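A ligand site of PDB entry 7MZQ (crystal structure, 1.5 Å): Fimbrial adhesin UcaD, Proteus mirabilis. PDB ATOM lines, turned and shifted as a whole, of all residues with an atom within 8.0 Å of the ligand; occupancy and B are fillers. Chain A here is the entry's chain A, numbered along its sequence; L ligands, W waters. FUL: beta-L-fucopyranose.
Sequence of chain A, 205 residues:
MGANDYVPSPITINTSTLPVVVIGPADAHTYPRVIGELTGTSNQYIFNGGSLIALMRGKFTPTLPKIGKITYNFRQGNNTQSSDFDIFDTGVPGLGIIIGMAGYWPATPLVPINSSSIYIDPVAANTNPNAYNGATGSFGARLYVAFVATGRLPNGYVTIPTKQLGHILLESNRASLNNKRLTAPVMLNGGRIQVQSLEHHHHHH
O of Gln 44 is in hydrogen-bond range of O3 of the ligand. NE2 of Gln 44 lies within hydrogen-bond range of O4 of the ligand, at 3.0 Å. An oxygen (O2) of the ligand sits at hydrogen-bond distance from the backbone NH (N) of Gly 140 (2.9 Å). NE1 of Trp 105 sits at hydrogen-bond distance from O4 of the ligand (3.1 Å).
OE1 of Gln 44 lies within hydrogen-bond range of OH of Tyr 45, 3.5 Å away. The guanidinium group (NH2) of Arg 142 lies within hydrogen-bond range of the backbone carbonyl oxygen (O) of Trp 105 (3.1 Å). The guanidinium group (NE) of Arg 142 lies within hydrogen-bond range of the backbone carbonyl oxygen (O) of Tyr 104, at 3.3 Å. The backbone carbonyl oxygen (O) of Phe 139 lies within hydrogen-bond range of the backbone NH (N) of Ile 46 (2.9 Å). The backbone carbonyl oxygen of Phe 47 is in hydrogen-bond range of the backbone NH of Phe 139 (2.9 Å). The backbone carbonyl oxygen (O) of Thr 136 lies within hydrogen-bond range of the backbone NH (N) of Ala 54, at 2.9 Å. The side-chain carboxylate (OD2) of Asp 121 lies within hydrogen-bond range of the side-chain amide nitrogen (ND2) of Asn 133, 2.9 Å away. The backbone carbonyl oxygen (O) of Met 56 is in hydrogen-bond range of the backbone NH (N) of Asn 133.
Merely in contact with the ligand: Tyr 104 (3.4 Å), Asn 133 (3.8 Å), Thr 136 (3.7 Å), Ser 138 (3.3 Å) and Phe 139 (3.4 Å). Eight residues have an atom within 4 Å of the ligand: Gln 44, Tyr 104, Trp 105, Asn 133, Thr 136, Ser 138, Phe 139 and Gly 140. Along chain A the residues within 4 Å of the ligand span positions 44 to 140.
Water W1 lies within hydrogen-bond range of O2 of the ligand, OD2 of Asp 121, O of Gly 140 and N of Tyr 104. Water W2 lies within hydrogen-bond range of an oxygen (O1) of the ligand (2.8 Å) and the backbone carbonyl oxygen of Gly 134 (2.8 Å).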
ATOM      1  N   ASN A  43      -2.982  22.003 -32.028  1.00  0.00           N
ATOM      2  CA  ASN A  43      -3.768  22.352 -30.851  1.00  0.00           C
ATOM      3  C   ASN A  43      -2.886  22.055 -29.650  1.00  0.00           C
ATOM      4  O   ASN A  43      -2.517  20.900 -29.430  1.00  0.00           O
ATOM      5  CB  ASN A  43      -5.083  21.576 -30.808  1.00  0.00           C
ATOM      6  CG  ASN A  43      -5.947  21.957 -29.635  1.00  0.00           C
ATOM      7  OD1 ASN A  43      -5.519  22.701 -28.741  1.00  0.00           O
ATOM      8  ND2 ASN A  43      -7.156  21.425 -29.580  1.00  0.00           N
ATOM      9  N   GLN A  44      -2.494  23.093 -28.910  1.00  0.00           N
ATOM     10  CA  GLN A  44      -1.620  22.933 -27.762  1.00  0.00           C
ATOM     11  C   GLN A  44      -2.334  22.250 -26.609  1.00  0.00           C
ATOM     12  O   GLN A  44      -1.665  21.653 -25.745  1.00  0.00           O
ATOM     13  CB  GLN A  44      -1.093  24.313 -27.352  1.00  0.00           C
ATOM     14  CG  GLN A  44       0.018  24.270 -26.335  1.00  0.00           C
ATOM     15  CD  GLN A  44       0.682  25.599 -26.113  1.00  0.00           C
ATOM     16  OE1 GLN A  44       0.211  26.636 -26.581  1.00  0.00           O
ATOM     17  NE2 GLN A  44       1.780  25.576 -25.371  1.00  0.00           N
ATOM     18  N   TYR A  45      -3.649  22.283 -26.570  1.00  0.00           N
ATOM     19  CA  TYR A  45      -4.432  21.908 -25.395  1.00  0.00           C
ATOM     20  C   TYR A  45      -5.465  20.867 -25.767  1.00  0.00           C
ATOM     21  O   TYR A  45      -6.659  21.019 -25.496  1.00  0.00           O
ATOM     22  CB  TYR A  45      -5.068  23.178 -24.792  1.00  0.00           C
ATOM     23  CG  TYR A  45      -4.038  24.220 -24.411  1.00  0.00           C
ATOM     24  CD1 TYR A  45      -3.133  23.992 -23.395  1.00  0.00           C
ATOM     25  CD2 TYR A  45      -3.959  25.420 -25.106  1.00  0.00           C
ATOM     26  CE1 TYR A  45      -2.175  24.919 -23.067  1.00  0.00           C
ATOM     27  CE2 TYR A  45      -2.993  26.377 -24.767  1.00  0.00           C
ATOM     28  CZ  TYR A  45      -2.111  26.090 -23.742  1.00  0.00           C
ATOM     29  OH  TYR A  45      -1.131  27.009 -23.377  1.00  0.00           O
ATOM     30  N   ILE A  46      -4.992  19.764 -26.353  1.00  0.00           N
ATOM     31  CA  ILE A  46      -5.891  18.636 -26.620  1.00  0.00           C
ATOM     32  C   ILE A  46      -6.359  18.016 -25.313  1.00  0.00           C
ATOM     33  O   ILE A  46      -7.528  17.642 -25.165  1.00  0.00           O
ATOM     34  CB  ILE A  46      -5.212  17.612 -27.540  1.00  0.00           C
ATOM     35  CG1 ILE A  46      -4.944  18.249 -28.913  1.00  0.00           C
ATOM     36  CG2 ILE A  46      -6.113  16.387 -27.708  1.00  0.00           C
ATOM     37  CD1 ILE A  46      -4.135  17.369 -29.849  1.00  0.00           C
ATOM     38  N   PHE A  47      -5.448  17.900 -24.334  1.00  0.00           N
ATOM     39  CA  PHE A  47      -5.834  17.524 -22.979  1.00  0.00           C
ATOM     40  C   PHE A  47      -5.291  18.603 -22.047  1.00  0.00           C
ATOM     41  O   PHE A  47      -4.120  18.968 -22.141  1.00  0.00           O
ATOM     42  CB  PHE A  47      -5.298  16.147 -22.554  1.00  0.00           C
ATOM     43  CG  PHE A  47      -5.758  15.031 -23.472  1.00  0.00           C
ATOM     44  CD1 PHE A  47      -7.041  14.496 -23.354  1.00  0.00           C
ATOM     45  CD2 PHE A  47      -4.915  14.526 -24.425  1.00  0.00           C
ATOM     46  CE1 PHE A  47      -7.462  13.506 -24.209  1.00  0.00           C
ATOM     47  CE2 PHE A  47      -5.343  13.528 -25.281  1.00  0.00           C
ATOM     48  CZ  PHE A  47      -6.608  13.017 -25.160  1.00  0.00           C
ATOM     49  N   ASN A  48      -6.146  19.127 -21.171  1.00  0.00           N
ATOM     50  CA  ASN A  48      -5.795  20.284 -20.347  1.00  0.00           C
ATOM     51  C   ASN A  48      -6.804  20.404 -19.225  1.00  0.00           C
ATOM     52  O   ASN A  48      -7.972  20.033 -19.399  1.00  0.00           O
ATOM     53  CB  ASN A  48      -5.785  21.556 -21.220  1.00  0.00           C
ATOM     54  CG  ASN A  48      -5.266  22.780 -20.512  1.00  0.00           C
ATOM     55  OD1 ASN A  48      -4.373  22.733 -19.677  1.00  0.00           O
ATOM     56  ND2 ASN A  48      -5.795  23.924 -20.909  1.00  0.00           N
ATOM     57  N   ALA A  54       1.498  16.341 -14.962  1.00  0.00           N
ATOM     58  CA  ALA A  54       1.553  14.916 -15.223  1.00  0.00           C
ATOM     59  C   ALA A  54       2.489  14.644 -16.395  1.00  0.00           C
ATOM     60  O   ALA A  54       2.665  15.486 -17.278  1.00  0.00           O
ATOM     61  CB  ALA A  54       0.161  14.351 -15.527  1.00  0.00           C
ATOM     62  N   MET A  56       2.652  12.609 -19.626  1.00  0.00           N
ATOM     63  CA  MET A  56       1.561  12.196 -20.502  1.00  0.00           C
ATOM     64  C   MET A  56       2.094  11.794 -21.867  1.00  0.00           C
ATOM     65  O   MET A  56       3.197  12.161 -22.271  1.00  0.00           O
ATOM     66  CB  MET A  56       0.542  13.344 -20.658  1.00  0.00           C
ATOM     67  CG  MET A  56      -0.170  13.682 -19.336  1.00  0.00           C
ATOM     68  SD  MET A  56      -1.338  15.068 -19.434  1.00  0.00           S
ATOM     69  CE  MET A  56      -0.179  16.432 -19.290  1.00  0.00           C
ATOM     70  N   ARG A  57       1.276  11.039 -22.585  1.00  0.00           N
ATOM     71  CA  ARG A  57       1.536  10.650 -23.962  1.00  0.00           C
ATOM     72  C   ARG A  57       0.202  10.431 -24.668  1.00  0.00           C
ATOM     73  O   ARG A  57      -0.831  10.219 -24.028  1.00  0.00           O
ATOM     74  CB  ARG A  57       2.393   9.391 -24.050  1.00  0.00           C
ATOM     75  CG  ARG A  57       1.748   8.150 -23.515  1.00  0.00           C
ATOM     76  CD  ARG A  57       2.750   7.021 -23.500  1.00  0.00           C
ATOM     77  NE  ARG A  57       2.205   5.795 -22.960  1.00  0.00           N
ATOM     78  CZ  ARG A  57       2.934   4.806 -22.489  1.00  0.00           C
ATOM     79  NH1 ARG A  57       4.251   4.884 -22.431  1.00  0.00           N
ATOM     80  NH2 ARG A  57       2.327   3.702 -22.067  1.00  0.00           N
ATOM     81  N   ALA A 102       2.193  14.730 -34.910  1.00  0.00           N
ATOM     82  CA  ALA A 102       3.418  14.988 -34.174  1.00  0.00           C
ATOM     83  C   ALA A 102       3.093  15.602 -32.830  1.00  0.00           C
ATOM     84  O   ALA A 102       1.980  16.070 -32.580  1.00  0.00           O
ATOM     85  CB  ALA A 102       4.363  15.914 -34.939  1.00  0.00           C
ATOM     86  N   GLY A 103       4.097  15.617 -31.949  1.00  0.00           N
ATOM     87  CA  GLY A 103       4.008  16.452 -30.765  1.00  0.00           C
ATOM     88  C   GLY A 103       3.818  17.917 -31.124  1.00  0.00           C
ATOM     89  O   GLY A 103       4.054  18.361 -32.253  1.00  0.00           O
ATOM     90  N   TYR A 104       3.335  18.680 -30.144  1.00  0.00           N
ATOM     91  CA  TYR A 104       3.053  20.086 -30.400  1.00  0.00           C
ATOM     92  C   TYR A 104       4.298  20.850 -30.824  1.00  0.00           C
ATOM     93  O   TYR A 104       4.247  21.664 -31.755  1.00  0.00           O
ATOM     94  CB  TYR A 104       2.436  20.738 -29.147  1.00  0.00           C
ATOM     95  CG  TYR A 104       2.126  22.196 -29.351  1.00  0.00           C
ATOM     96  CD1 TYR A 104       1.062  22.599 -30.142  1.00  0.00           C
ATOM     97  CD2 TYR A 104       2.926  23.184 -28.789  1.00  0.00           C
ATOM     98  CE1 TYR A 104       0.799  23.939 -30.367  1.00  0.00           C
ATOM     99  CE2 TYR A 104       2.662  24.510 -29.004  1.00  0.00           C
ATOM    100  CZ  TYR A 104       1.599  24.886 -29.782  1.00  0.00           C
ATOM    101  OH  TYR A 104       1.327  26.218 -29.999  1.00  0.00           O
ATOM    102  N   TRP A 105       5.391  20.673 -30.113  1.00  0.00           N
ATOM    103  CA  TRP A 105       6.571  21.497 -30.351  1.00  0.00           C
ATOM    104  C   TRP A 105       7.300  21.052 -31.619  1.00  0.00           C
ATOM    105  O   TRP A 105       7.431  19.859 -31.886  1.00  0.00           O
ATOM    106  CB  TRP A 105       7.492  21.443 -29.135  1.00  0.00           C
ATOM    107  CG  TRP A 105       6.817  22.032 -27.935  1.00  0.00           C
ATOM    108  CD1 TRP A 105       6.331  21.355 -26.867  1.00  0.00           C
ATOM    109  CD2 TRP A 105       6.489  23.415 -27.735  1.00  0.00           C
ATOM    110  NE1 TRP A 105       5.731  22.228 -25.989  1.00  0.00           N
ATOM    111  CE2 TRP A 105       5.817  23.498 -26.499  1.00  0.00           C
ATOM    112  CE3 TRP A 105       6.707  24.579 -28.462  1.00  0.00           C
ATOM    113  CZ2 TRP A 105       5.384  24.716 -25.963  1.00  0.00           C
ATOM    114  CZ3 TRP A 105       6.259  25.786 -27.949  1.00  0.00           C
ATOM    115  CH2 TRP A 105       5.605  25.844 -26.707  1.00  0.00           C
ATOM    116  N   THR A 108       9.642  17.940 -32.499  1.00  0.00           N
ATOM    117  CA  THR A 108       9.226  16.543 -32.524  1.00  0.00           C
ATOM    118  C   THR A 108       8.862  16.145 -33.964  1.00  0.00           C
ATOM    119  O   THR A 108       8.376  16.969 -34.733  1.00  0.00           O
ATOM    120  CB  THR A 108       8.016  16.301 -31.608  1.00  0.00           C
ATOM    121  OG1 THR A 108       6.906  17.087 -32.023  1.00  0.00           O
ATOM    122  CG2 THR A 108       8.358  16.639 -30.159  1.00  0.00           C
ATOM    123  N   ASP A 121       3.371  11.133 -29.687  1.00  0.00           N
ATOM    124  CA  ASP A 121       4.273  11.912 -28.845  1.00  0.00           C
ATOM    125  C   ASP A 121       4.227  11.320 -27.447  1.00  0.00           C
ATOM    126  O   ASP A 121       3.133  11.127 -26.897  1.00  0.00           O
ATOM    127  CB  ASP A 121       3.883  13.399 -28.813  1.00  0.00           C
ATOM    128  CG  ASP A 121       4.964  14.290 -28.221  1.00  0.00           C
ATOM    129  OD1 ASP A 121       6.157  14.079 -28.509  1.00  0.00           O
ATOM    130  OD2 ASP A 121       4.611  15.237 -27.489  1.00  0.00           O
ATOM    131  N   ASN A 133       5.989  12.044 -22.084  1.00  0.00           N
ATOM    132  CA  ASN A 133       6.475  13.413 -22.141  1.00  0.00           C
ATOM    133  C   ASN A 133       6.908  13.893 -20.761  1.00  0.00           C
ATOM    134  O   ASN A 133       6.391  13.467 -19.729  1.00  0.00           O
ATOM    135  CB  ASN A 133       5.408  14.390 -22.640  1.00  0.00           C
ATOM    136  CG  ASN A 133       5.216  14.346 -24.131  1.00  0.00           C
ATOM    137  OD1 ASN A 133       6.019  13.766 -24.861  1.00  0.00           O
ATOM    138  ND2 ASN A 133       4.136  14.981 -24.600  1.00  0.00           N
ATOM    139  N   GLY A 134       7.850  14.834 -20.749  1.00  0.00           N
ATOM    140  CA  GLY A 134       8.162  15.533 -19.520  1.00  0.00           C
ATOM    141  C   GLY A 134       6.944  16.138 -18.861  1.00  0.00           C
ATOM    142  O   GLY A 134       6.003  16.575 -19.549  1.00  0.00           O
ATOM    143  N   ALA A 135       6.958  16.221 -17.535  1.00  0.00           N
ATOM    144  CA  ALA A 135       5.784  16.646 -16.790  1.00  0.00           C
ATOM    145  C   ALA A 135       5.394  18.080 -17.128  1.00  0.00           C
ATOM    146  O   ALA A 135       6.241  18.978 -17.212  1.00  0.00           O
ATOM    147  CB  ALA A 135       6.039  16.543 -15.282  1.00  0.00           C
ATOM    148  N   THR A 136       4.104  18.282 -17.292  1.00  0.00           N
ATOM    149  CA  THR A 136       3.536  19.594 -17.607  1.00  0.00           C
ATOM    150  C   THR A 136       2.029  19.510 -17.414  1.00  0.00           C
ATOM    151  O   THR A 136       1.481  18.497 -16.962  1.00  0.00           O
ATOM    152  CB  THR A 136       3.946  20.032 -19.011  1.00  0.00           C
ATOM    153  OG1 THR A 136       3.496  21.384 -19.235  1.00  0.00           O
ATOM    154  CG2 THR A 136       3.403  19.120 -20.070  1.00  0.00           C
ATOM    155  N   GLY A 137       1.342  20.599 -17.736  1.00  0.00           N
ATOM    156  CA  GLY A 137      -0.070  20.690 -17.499  1.00  0.00           C
ATOM    157  C   GLY A 137      -0.956  20.492 -18.699  1.00  0.00           C
ATOM    158  O   GLY A 137      -2.175  20.682 -18.583  1.00  0.00           O
ATOM    159  N   SER A 138      -0.413  20.093 -19.843  1.00  0.00           N
ATOM    160  CA  SER A 138      -1.247  19.877 -21.007  1.00  0.00           C
ATOM    161  C   SER A 138      -0.546  18.943 -21.979  1.00  0.00           C
ATOM    162  O   SER A 138       0.662  18.723 -21.889  1.00  0.00           O
ATOM    163  CB  SER A 138      -1.598  21.192 -21.711  1.00  0.00           C
ATOM    164  OG  SER A 138      -0.422  21.874 -22.075  1.00  0.00           O
ATOM    165  N   PHE A 139      -1.337  18.406 -22.912  1.00  0.00           N
ATOM    166  CA  PHE A 139      -0.824  17.603 -24.037  1.00  0.00           C
ATOM    167  C   PHE A 139      -1.439  18.163 -25.320  1.00  0.00           C
ATOM    168  O   PHE A 139      -2.655  18.335 -25.378  1.00  0.00           O
ATOM    169  CB  PHE A 139      -1.201  16.129 -23.881  1.00  0.00           C
ATOM    170  CG  PHE A 139      -0.746  15.272 -25.038  1.00  0.00           C
ATOM    171  CD1 PHE A 139      -1.548  15.129 -26.167  1.00  0.00           C
ATOM    172  CD2 PHE A 139       0.480  14.661 -25.009  1.00  0.00           C
ATOM    173  CE1 PHE A 139      -1.113  14.364 -27.243  1.00  0.00           C
ATOM    174  CE2 PHE A 139       0.926  13.899 -26.072  1.00  0.00           C
ATOM    175  CZ  PHE A 139       0.118  13.748 -27.202  1.00  0.00           C
ATOM    176  N   GLY A 140      -0.602  18.450 -26.308  1.00  0.00           N
ATOM    177  CA  GLY A 140      -1.057  18.908 -27.603  1.00  0.00           C
ATOM    178  C   GLY A 140      -0.405  18.143 -28.745  1.00  0.00           C
ATOM    179  O   GLY A 140       0.368  17.205 -28.535  1.00  0.00           O
ATOM    180  N   ALA A 141      -0.736  18.575 -29.964  1.00  0.00           N
ATOM    181  CA  ALA A 141      -0.228  17.868 -31.128  1.00  0.00           C
ATOM    182  C   ALA A 141      -0.337  18.728 -32.378  1.00  0.00           C
ATOM    183  O   ALA A 141      -0.987  19.784 -32.366  1.00  0.00           O
ATOM    184  CB  ALA A 141      -0.989  16.548 -31.355  1.00  0.00           C
ATOM    185  N   ARG A 142       0.325  18.267 -33.435  1.00  0.00           N
ATOM    186  CA  ARG A 142       0.219  18.778 -34.796  1.00  0.00           C
ATOM    187  C   ARG A 142      -0.413  17.681 -35.658  1.00  0.00           C
ATOM    188  O   ARG A 142      -0.146  16.490 -35.452  1.00  0.00           O
ATOM    189  CB  ARG A 142       1.577  19.182 -35.383  1.00  0.00           C
ATOM    190  CG  ARG A 142       2.138  20.398 -34.662  1.00  0.00           C
ATOM    191  CD  ARG A 142       3.473  20.821 -35.173  1.00  0.00           C
ATOM    192  NE  ARG A 142       4.489  20.001 -34.543  1.00  0.00           N
ATOM    193  CZ  ARG A 142       5.432  19.320 -35.177  1.00  0.00           C
ATOM    194  NH1 ARG A 142       5.490  19.283 -36.497  1.00  0.00           N
ATOM    195  NH2 ARG A 142       6.321  18.657 -34.467  1.00  0.00           N
HETATM  196  C1  FUL L   1       3.691  19.510 -23.921  1.00  0.00           C
HETATM  197  C2  FUL L   1       2.744  19.715 -25.102  1.00  0.00           C
HETATM  198  O2  FUL L   1       2.170  18.459 -25.430  1.00  0.00           O
HETATM  199  C3  FUL L   1       1.648  20.676 -24.819  1.00  0.00           C
HETATM  200  O3  FUL L   1       1.029  21.029 -26.100  1.00  0.00           O
HETATM  201  C4  FUL L   1       2.100  21.961 -24.205  1.00  0.00           C
HETATM  202  O4  FUL L   1       2.772  22.764 -25.181  1.00  0.00           O
HETATM  203  C5  FUL L   1       3.101  21.676 -23.097  1.00  0.00           C
HETATM  204  C6  FUL L   1       3.756  22.926 -22.592  1.00  0.00           C
HETATM  205  O5  FUL L   1       4.168  20.781 -23.538  1.00  0.00           O
HETATM  206  O1  FUL L   1       4.722  18.714 -24.253  1.00  0.00           O
HETATM  207  O   HOH W   1       2.846  17.192 -27.568  1.00  0.00           O
HETATM  208  O   HOH W   2       6.228  17.862 -22.068  1.00  0.00           O
